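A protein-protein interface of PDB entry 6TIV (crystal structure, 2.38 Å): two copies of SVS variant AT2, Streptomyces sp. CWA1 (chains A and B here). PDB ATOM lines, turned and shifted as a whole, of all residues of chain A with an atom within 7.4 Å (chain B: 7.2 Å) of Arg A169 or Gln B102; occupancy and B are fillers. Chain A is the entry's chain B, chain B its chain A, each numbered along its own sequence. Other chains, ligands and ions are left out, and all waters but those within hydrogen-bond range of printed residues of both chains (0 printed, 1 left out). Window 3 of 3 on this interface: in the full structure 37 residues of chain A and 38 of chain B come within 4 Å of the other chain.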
ATOM      1  N   ARG A  99      -7.098 -24.940 -24.162  1.00  0.00           N
ATOM      2  CA  ARG A  99      -7.520 -23.553 -23.845  1.00  0.00           C
ATOM      3  C   ARG A  99      -7.522 -22.728 -25.131  1.00  0.00           C
ATOM      4  O   ARG A  99      -6.696 -22.966 -26.012  1.00  0.00           O
ATOM      5  CB  ARG A  99      -6.577 -22.894 -22.837  1.00  0.00           C
ATOM      6  CG  ARG A  99      -6.426 -23.627 -21.515  1.00  0.00           C
ATOM      7  CD  ARG A  99      -7.754 -24.071 -20.921  1.00  0.00           C
ATOM      8  NE  ARG A  99      -8.667 -22.990 -20.522  1.00  0.00           N
ATOM      9  CZ  ARG A  99      -9.981 -23.164 -20.326  1.00  0.00           C
ATOM     10  NH1 ARG A  99     -10.513 -24.367 -20.488  1.00  0.00           N
ATOM     11  NH2 ARG A  99     -10.747 -22.148 -19.962  1.00  0.00           N
ATOM     12  N   PRO A 100      -8.424 -21.720 -25.247  1.00  0.00           N
ATOM     13  CA  PRO A 100      -8.420 -20.773 -26.355  1.00  0.00           C
ATOM     14  C   PRO A 100      -7.050 -20.178 -26.693  1.00  0.00           C
ATOM     15  O   PRO A 100      -6.705 -20.135 -27.875  1.00  0.00           O
ATOM     16  CB  PRO A 100      -9.344 -19.652 -25.884  1.00  0.00           C
ATOM     17  CG  PRO A 100     -10.307 -20.353 -24.961  1.00  0.00           C
ATOM     18  CD  PRO A 100      -9.490 -21.425 -24.278  1.00  0.00           C
ATOM     19  N   TRP A 162     -13.861 -19.973 -32.089  1.00  0.00           N
ATOM     20  CA  TRP A 162     -15.039 -19.245 -31.548  1.00  0.00           C
ATOM     21  C   TRP A 162     -15.757 -20.141 -30.535  1.00  0.00           C
ATOM     22  O   TRP A 162     -16.093 -19.660 -29.398  1.00  0.00           O
ATOM     23  CB  TRP A 162     -15.927 -18.854 -32.706  1.00  0.00           C
ATOM     24  CG  TRP A 162     -17.049 -17.938 -32.417  1.00  0.00           C
ATOM     25  CD1 TRP A 162     -17.555 -17.574 -31.208  1.00  0.00           C
ATOM     26  CD2 TRP A 162     -17.881 -17.319 -33.405  1.00  0.00           C
ATOM     27  NE1 TRP A 162     -18.600 -16.703 -31.381  1.00  0.00           N
ATOM     28  CE2 TRP A 162     -18.853 -16.574 -32.717  1.00  0.00           C
ATOM     29  CE3 TRP A 162     -17.908 -17.348 -34.796  1.00  0.00           C
ATOM     30  CZ2 TRP A 162     -19.812 -15.830 -33.373  1.00  0.00           C
ATOM     31  CZ3 TRP A 162     -18.870 -16.625 -35.455  1.00  0.00           C
ATOM     32  CH2 TRP A 162     -19.820 -15.894 -34.753  1.00  0.00           C
ATOM     33  N   GLN A 163     -15.930 -21.412 -30.887  1.00  0.00           N
ATOM     34  CA  GLN A 163     -16.701 -22.382 -30.063  1.00  0.00           C
ATOM     35  C   GLN A 163     -15.949 -22.712 -28.767  1.00  0.00           C
ATOM     36  O   GLN A 163     -16.581 -22.618 -27.720  1.00  0.00           O
ATOM     37  CB  GLN A 163     -16.965 -23.649 -30.851  1.00  0.00           C
ATOM     38  CG  GLN A 163     -17.938 -24.603 -30.202  1.00  0.00           C
ATOM     39  CD  GLN A 163     -17.948 -25.760 -31.163  1.00  0.00           C
ATOM     40  OE1 GLN A 163     -17.055 -26.615 -31.099  1.00  0.00           O
ATOM     41  NE2 GLN A 163     -18.868 -25.702 -32.133  1.00  0.00           N
ATOM     42  N   ILE A 164     -14.649 -23.032 -28.856  1.00  0.00           N
ATOM     43  CA  ILE A 164     -13.740 -23.218 -27.696  1.00  0.00           C
ATOM     44  C   ILE A 164     -13.727 -21.944 -26.824  1.00  0.00           C
ATOM     45  O   ILE A 164     -13.685 -22.072 -25.588  1.00  0.00           O
ATOM     46  CB  ILE A 164     -12.337 -23.635 -28.172  1.00  0.00           C
ATOM     47  CG1 ILE A 164     -12.365 -24.999 -28.863  1.00  0.00           C
ATOM     48  CG2 ILE A 164     -11.362 -23.595 -27.010  1.00  0.00           C
ATOM     49  CD1 ILE A 164     -11.047 -25.415 -29.519  1.00  0.00           C
ATOM     50  N   GLY A 165     -13.763 -20.756 -27.414  1.00  0.00           N
ATOM     51  CA  GLY A 165     -13.796 -19.485 -26.655  1.00  0.00           C
ATOM     52  C   GLY A 165     -15.093 -19.361 -25.863  1.00  0.00           C
ATOM     53  O   GLY A 165     -15.058 -18.969 -24.706  1.00  0.00           O
ATOM     54  N   ASN A 166     -16.218 -19.681 -26.474  1.00  0.00           N
ATOM     55  CA  ASN A 166     -17.546 -19.552 -25.829  1.00  0.00           C
ATOM     56  C   ASN A 166     -17.617 -20.535 -24.675  1.00  0.00           C
ATOM     57  O   ASN A 166     -18.064 -20.148 -23.598  1.00  0.00           O
ATOM     58  CB  ASN A 166     -18.714 -19.859 -26.755  1.00  0.00           C
ATOM     59  CG  ASN A 166     -18.971 -18.776 -27.775  1.00  0.00           C
ATOM     60  OD1 ASN A 166     -18.413 -17.685 -27.684  1.00  0.00           O
ATOM     61  ND2 ASN A 166     -19.798 -19.096 -28.749  1.00  0.00           N
ATOM     62  N   GLN A 167     -17.115 -21.735 -24.879  1.00  0.00           N
ATOM     63  CA  GLN A 167     -17.184 -22.791 -23.856  1.00  0.00           C
ATOM     64  C   GLN A 167     -16.309 -22.406 -22.650  1.00  0.00           C
ATOM     65  O   GLN A 167     -16.794 -22.594 -21.505  1.00  0.00           O
ATOM     66  CB  GLN A 167     -16.869 -24.146 -24.481  1.00  0.00           C
ATOM     67  CG  GLN A 167     -15.835 -24.930 -23.692  1.00  0.00           C
ATOM     68  CD  GLN A 167     -16.320 -26.299 -23.318  1.00  0.00           C
ATOM     69  OE1 GLN A 167     -16.903 -27.012 -24.138  1.00  0.00           O
ATOM     70  NE2 GLN A 167     -16.058 -26.663 -22.070  1.00  0.00           N
ATOM     71  N   ALA A 168     -15.084 -21.926 -22.876  1.00  0.00           N
ATOM     72  CA  ALA A 168     -14.137 -21.572 -21.808  1.00  0.00           C
ATOM     73  C   ALA A 168     -14.716 -20.449 -20.948  1.00  0.00           C
ATOM     74  O   ALA A 168     -14.457 -20.452 -19.757  1.00  0.00           O
ATOM     75  CB  ALA A 168     -12.829 -21.171 -22.407  1.00  0.00           C
ATOM     76  N   ARG A 169     -15.422 -19.509 -21.550  1.00  0.00           N
ATOM     77  CA  ARG A 169     -15.979 -18.320 -20.864  1.00  0.00           C
ATOM     78  C   ARG A 169     -17.341 -18.598 -20.200  1.00  0.00           C
ATOM     79  O   ARG A 169     -17.854 -17.662 -19.583  1.00  0.00           O
ATOM     80  CB  ARG A 169     -16.303 -17.205 -21.865  1.00  0.00           C
ATOM     81  CG  ARG A 169     -15.105 -16.547 -22.518  1.00  0.00           C
ATOM     82  CD  ARG A 169     -15.603 -15.726 -23.700  1.00  0.00           C
ATOM     83  NE  ARG A 169     -16.558 -14.688 -23.323  1.00  0.00           N
ATOM     84  CZ  ARG A 169     -17.365 -14.061 -24.187  1.00  0.00           C
ATOM     85  NH1 ARG A 169     -17.377 -14.397 -25.473  1.00  0.00           N
ATOM     86  NH2 ARG A 169     -18.182 -13.123 -23.753  1.00  0.00           N
ATOM     87  N   GLY A 170     -17.959 -19.757 -20.435  1.00  0.00           N
ATOM     88  CA  GLY A 170     -19.397 -19.999 -20.221  1.00  0.00           C
ATOM     89  C   GLY A 170     -20.295 -18.973 -20.905  1.00  0.00           C
ATOM     90  O   GLY A 170     -21.163 -18.400 -20.224  1.00  0.00           O
ATOM     91  N   HIS A 171     -20.107 -18.725 -22.201  1.00  0.00           N
ATOM     92  CA  HIS A 171     -21.043 -17.939 -23.038  1.00  0.00           C
ATOM     93  C   HIS A 171     -21.863 -18.913 -23.894  1.00  0.00           C
ATOM     94  O   HIS A 171     -21.265 -19.622 -24.718  1.00  0.00           O
ATOM     95  CB  HIS A 171     -20.278 -16.911 -23.873  1.00  0.00           C
ATOM     96  CG  HIS A 171     -21.132 -16.048 -24.746  1.00  0.00           C
ATOM     97  ND1 HIS A 171     -21.803 -14.947 -24.267  1.00  0.00           N
ATOM     98  CD2 HIS A 171     -21.398 -16.091 -26.075  1.00  0.00           C
ATOM     99  CE1 HIS A 171     -22.464 -14.365 -25.250  1.00  0.00           C
ATOM    100  NE2 HIS A 171     -22.247 -15.050 -26.364  1.00  0.00           N
ATOM    101  N   MET A 172     -23.171 -18.986 -23.641  1.00  0.00           N
ATOM    102  CA  MET A 172     -24.165 -19.631 -24.528  1.00  0.00           C
ATOM    103  C   MET A 172     -24.589 -18.567 -25.528  1.00  0.00           C
ATOM    104  O   MET A 172     -25.189 -17.561 -25.152  1.00  0.00           O
ATOM    105  CB  MET A 172     -25.396 -20.153 -23.776  1.00  0.00           C
ATOM    106  CG  MET A 172     -26.364 -20.972 -24.638  1.00  0.00           C
ATOM    107  SD  MET A 172     -25.701 -22.519 -25.352  1.00  0.00           S
ATOM    108  CE  MET A 172     -25.089 -23.388 -23.906  1.00  0.00           C
ATOM    109  N   PRO B  95      -9.495  -4.688 -23.916  1.00  0.00           N
ATOM    110  CA  PRO B  95      -9.549  -5.733 -22.879  1.00  0.00           C
ATOM    111  C   PRO B  95      -9.492  -7.108 -23.559  1.00  0.00           C
ATOM    112  O   PRO B  95      -9.233  -8.101 -22.903  1.00  0.00           O
ATOM    113  CB  PRO B  95     -10.921  -5.514 -22.229  1.00  0.00           C
ATOM    114  CG  PRO B  95     -11.169  -4.033 -22.401  1.00  0.00           C
ATOM    115  CD  PRO B  95     -10.559  -3.694 -23.747  1.00  0.00           C
ATOM    116  N   LEU B  96      -9.740  -7.096 -24.871  1.00  0.00           N
ATOM    117  CA  LEU B  96      -9.665  -8.276 -25.768  1.00  0.00           C
ATOM    118  C   LEU B  96      -8.209  -8.613 -26.093  1.00  0.00           C
ATOM    119  O   LEU B  96      -7.988  -9.740 -26.531  1.00  0.00           O
ATOM    120  CB  LEU B  96     -10.462  -8.006 -27.045  1.00  0.00           C
ATOM    121  CG  LEU B  96     -11.941  -8.365 -26.972  1.00  0.00           C
ATOM    122  CD1 LEU B  96     -12.669  -7.552 -25.921  1.00  0.00           C
ATOM    123  CD2 LEU B  96     -12.589  -8.169 -28.322  1.00  0.00           C
ATOM    124  N   ARG B  99      -7.365 -11.404 -23.990  1.00  0.00           N
ATOM    125  CA  ARG B  99      -8.609 -12.184 -23.735  1.00  0.00           C
ATOM    126  C   ARG B  99      -8.970 -12.926 -25.024  1.00  0.00           C
ATOM    127  O   ARG B  99      -9.887 -12.553 -25.755  1.00  0.00           O
ATOM    128  CB  ARG B  99      -9.687 -11.261 -23.155  1.00  0.00           C
ATOM    129  CG  ARG B  99      -9.329 -10.636 -21.805  1.00  0.00           C
ATOM    130  CD  ARG B  99      -9.031 -11.606 -20.680  1.00  0.00           C
ATOM    131  NE  ARG B  99     -10.248 -12.298 -20.277  1.00  0.00           N
ATOM    132  CZ  ARG B  99     -11.121 -11.894 -19.344  1.00  0.00           C
ATOM    133  NH1 ARG B  99     -10.913 -10.792 -18.640  1.00  0.00           N
ATOM    134  NH2 ARG B  99     -12.210 -12.618 -19.122  1.00  0.00           N
ATOM    135  N   PRO B 100      -8.210 -13.995 -25.348  1.00  0.00           N
ATOM    136  CA  PRO B 100      -8.370 -14.724 -26.610  1.00  0.00           C
ATOM    137  C   PRO B 100      -9.763 -15.322 -26.776  1.00  0.00           C
ATOM    138  O   PRO B 100     -10.275 -15.302 -27.919  1.00  0.00           O
ATOM    139  CB  PRO B 100      -7.361 -15.876 -26.600  1.00  0.00           C
ATOM    140  CG  PRO B 100      -6.717 -15.830 -25.205  1.00  0.00           C
ATOM    141  CD  PRO B 100      -7.109 -14.527 -24.533  1.00  0.00           C
ATOM    142  N   ALA B 101     -10.353 -15.832 -25.688  1.00  0.00           N
ATOM    143  CA  ALA B 101     -11.719 -16.420 -25.752  1.00  0.00           C
ATOM    144  C   ALA B 101     -12.715 -15.366 -26.254  1.00  0.00           C
ATOM    145  O   ALA B 101     -13.501 -15.688 -27.145  1.00  0.00           O
ATOM    146  CB  ALA B 101     -12.130 -17.004 -24.437  1.00  0.00           C
ATOM    147  N   GLN B 102     -12.624 -14.125 -25.785  1.00  0.00           N
ATOM    148  CA  GLN B 102     -13.543 -13.046 -26.218  1.00  0.00           C
ATOM    149  C   GLN B 102     -13.185 -12.573 -27.623  1.00  0.00           C
ATOM    150  O   GLN B 102     -14.113 -12.302 -28.369  1.00  0.00           O
ATOM    151  CB  GLN B 102     -13.512 -11.865 -25.255  1.00  0.00           C
ATOM    152  CG  GLN B 102     -14.174 -12.197 -23.948  1.00  0.00           C
ATOM    153  CD  GLN B 102     -14.162 -11.032 -22.999  1.00  0.00           C
ATOM    154  OE1 GLN B 102     -14.778  -9.993 -23.277  1.00  0.00           O
ATOM    155  NE2 GLN B 102     -13.467 -11.221 -21.881  1.00  0.00           N
ATOM    156  N   PHE B 103     -11.899 -12.441 -27.954  1.00  0.00           N
ATOM    157  CA  PHE B 103     -11.460 -11.990 -29.301  1.00  0.00           C
ATOM    158  C   PHE B 103     -11.987 -12.968 -30.354  1.00  0.00           C
ATOM    159  O   PHE B 103     -12.514 -12.524 -31.377  1.00  0.00           O
ATOM    160  CB  PHE B 103      -9.939 -11.843 -29.409  1.00  0.00           C
ATOM    161  CG  PHE B 103      -9.535 -11.238 -30.731  1.00  0.00           C
ATOM    162  CD1 PHE B 103      -9.675  -9.880 -30.941  1.00  0.00           C
ATOM    163  CD2 PHE B 103      -9.145 -12.036 -31.792  1.00  0.00           C
ATOM    164  CE1 PHE B 103      -9.364  -9.316 -32.160  1.00  0.00           C
ATOM    165  CE2 PHE B 103      -8.816 -11.463 -33.009  1.00  0.00           C
ATOM    166  CZ  PHE B 103      -8.967 -10.113 -33.204  1.00  0.00           C
ATOM    167  N   ASN B 104     -11.924 -14.272 -30.087  1.00  0.00           N
ATOM    168  CA  ASN B 104     -12.388 -15.303 -31.059  1.00  0.00           C
ATOM    169  C   ASN B 104     -13.850 -15.028 -31.439  1.00  0.00           C
ATOM    170  O   ASN B 104     -14.199 -15.154 -32.619  1.00  0.00           O
ATOM    171  CB  ASN B 104     -12.148 -16.693 -30.500  1.00  0.00           C
ATOM    172  CG  ASN B 104     -10.679 -17.055 -30.362  1.00  0.00           C
ATOM    173  OD1 ASN B 104      -9.808 -16.284 -30.712  1.00  0.00           O
ATOM    174  ND2 ASN B 104     -10.391 -18.237 -29.863  1.00  0.00           N
ATOM    175  N   ALA B 105     -14.700 -14.623 -30.498  1.00  0.00           N
ATOM    176  CA  ALA B 105     -16.126 -14.360 -30.793  1.00  0.00           C
ATOM    177  C   ALA B 105     -16.229 -13.082 -31.630  1.00  0.00           C
ATOM    178  O   ALA B 105     -16.932 -13.105 -32.691  1.00  0.00           O
ATOM    179  CB  ALA B 105     -16.934 -14.266 -29.526  1.00  0.00           C
ATOM    180  N   LEU B 106     -15.540 -12.012 -31.205  1.00  0.00           N
ATOM    181  CA  LEU B 106     -15.519 -10.725 -31.964  1.00  0.00           C
ATOM    182  C   LEU B 106     -15.032 -10.944 -33.412  1.00  0.00           C
ATOM    183  O   LEU B 106     -15.624 -10.386 -34.323  1.00  0.00           O
ATOM    184  CB  LEU B 106     -14.622  -9.711 -31.248  1.00  0.00           C
ATOM    185  CG  LEU B 106     -14.478  -8.391 -31.997  1.00  0.00           C
ATOM    186  CD1 LEU B 106     -15.790  -7.631 -32.041  1.00  0.00           C
ATOM    187  CD2 LEU B 106     -13.407  -7.529 -31.370  1.00  0.00           C
ATOM    188  N   ALA B 107     -13.944 -11.683 -33.597  1.00  0.00           N
ATOM    189  CA  ALA B 107     -13.372 -11.990 -34.921  1.00  0.00           C
ATOM    190  C   ALA B 107     -14.437 -12.666 -35.774  1.00  0.00           C
ATOM    191  O   ALA B 107     -14.552 -12.346 -36.968  1.00  0.00           O
ATOM    192  CB  ALA B 107     -12.148 -12.873 -34.776  1.00  0.00           C
ATOM    193  N   GLY B 108     -15.184 -13.574 -35.162  1.00  0.00           N
ATOM    194  CA  GLY B 108     -16.274 -14.309 -35.818  1.00  0.00           C
ATOM    195  C   GLY B 108     -17.408 -13.378 -36.192  1.00  0.00           C
ATOM    196  O   GLY B 108     -17.817 -13.430 -37.375  1.00  0.00           O
ATOM    197  N   ARG B 109     -17.834 -12.505 -35.282  1.00  0.00           N
ATOM    198  CA  ARG B 109     -18.926 -11.541 -35.589  1.00  0.00           C
ATOM    199  C   ARG B 109     -18.454 -10.542 -36.665  1.00  0.00           C
ATOM    200  O   ARG B 109     -19.146 -10.383 -37.689  1.00  0.00           O
ATOM    201  CB  ARG B 109     -19.502 -10.867 -34.336  1.00  0.00           C
ATOM    202  CG  ARG B 109     -20.303 -11.801 -33.429  1.00  0.00           C
ATOM    203  CD  ARG B 109     -21.034 -11.147 -32.252  1.00  0.00           C
ATOM    204  NE  ARG B 109     -20.185 -10.170 -31.611  1.00  0.00           N
ATOM    205  CZ  ARG B 109     -19.265 -10.451 -30.677  1.00  0.00           C
ATOM    206  NH1 ARG B 109     -19.114 -11.701 -30.255  1.00  0.00           N
ATOM    207  NH2 ARG B 109     -18.498  -9.481 -30.178  1.00  0.00           N
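NH2 of Arg B99 sits close to NE2 of Gln B102, at 3.3 Å. O of Pro B100 sits close to OD1 of Asn B104 (3.0 Å). O of Trp A162 sits close to OD1 of Asn A166, 3.5 Å away.
Of the 13 printed residues of chain B, 6 touch a printed residue of chain A. Hydrophobic or aromatic side chains of chain A within 4 Å of the printed part of chain B: Pro A100 and Trp A162. Among the printed residues, 8 pairs touch across the chains. Among the printed residues, no Asp or Glu carboxylate lies within 4 Å of a Lys or Arg side-chain nitrogen of the other chain.
Positions printed for both chains: 99 and 100. Of the 8 pairs that touch across the chains among the printed residues, none has its exchanged pair printed and touching as well.
Arg A169 touches just these residues of chain B: Ala B101 and Gln B102. Printed residues of chain A within 4 Å of Gln B102: Arg A169. Ala B101 touches just these residues of chain A: Pro A100 (3.8 Å), Gly A165 (3.5 Å) and Arg A169 (3.6 Å). Of the printed residues of chain B, Pro A100 touches Ala B101 (3.8 Å). Of the printed residues of chain A, Arg B109 touches Trp A162. Of the printed residues of chain A, Gly B108 touches Trp A162. Printed residues of chain A within 4 Å of Asn B104: Trp A162. Of the printed residues of chain B, Trp A162 touches Asn B104, Ala B105, Gly B108 and Arg B109. Arg A99 touches none of the printed residues of chain B. The nearest residue of chain B that does not touch Arg A169 is Ala B105 (4.1 Å). The nearest residue of chain A that does not touch Gln B102 is Gly A165 (5.5 Å). The nearest printed residue of chain A that does not touch Asn B104 is Pro A100 (4.4 Å).
Pro A100 touches Ala B101. Trp A162 touches Asn B104 (CG to O, 3.99 Å). Ala B105 touches Trp A162 (CA to NE1, 3.5 Å). CA of Gly B108 touches CZ3 of Trp A162, 3.5 Å away. Trp A162 touches Arg B109 (CH2 to N, 3.96 Å). Ala B101 touches Gly A165 (CB to O, 3.5 Å). Arg A169 touches Ala B101 (CG to CB, 3.6 Å). Arg A169 touches Gln B102.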
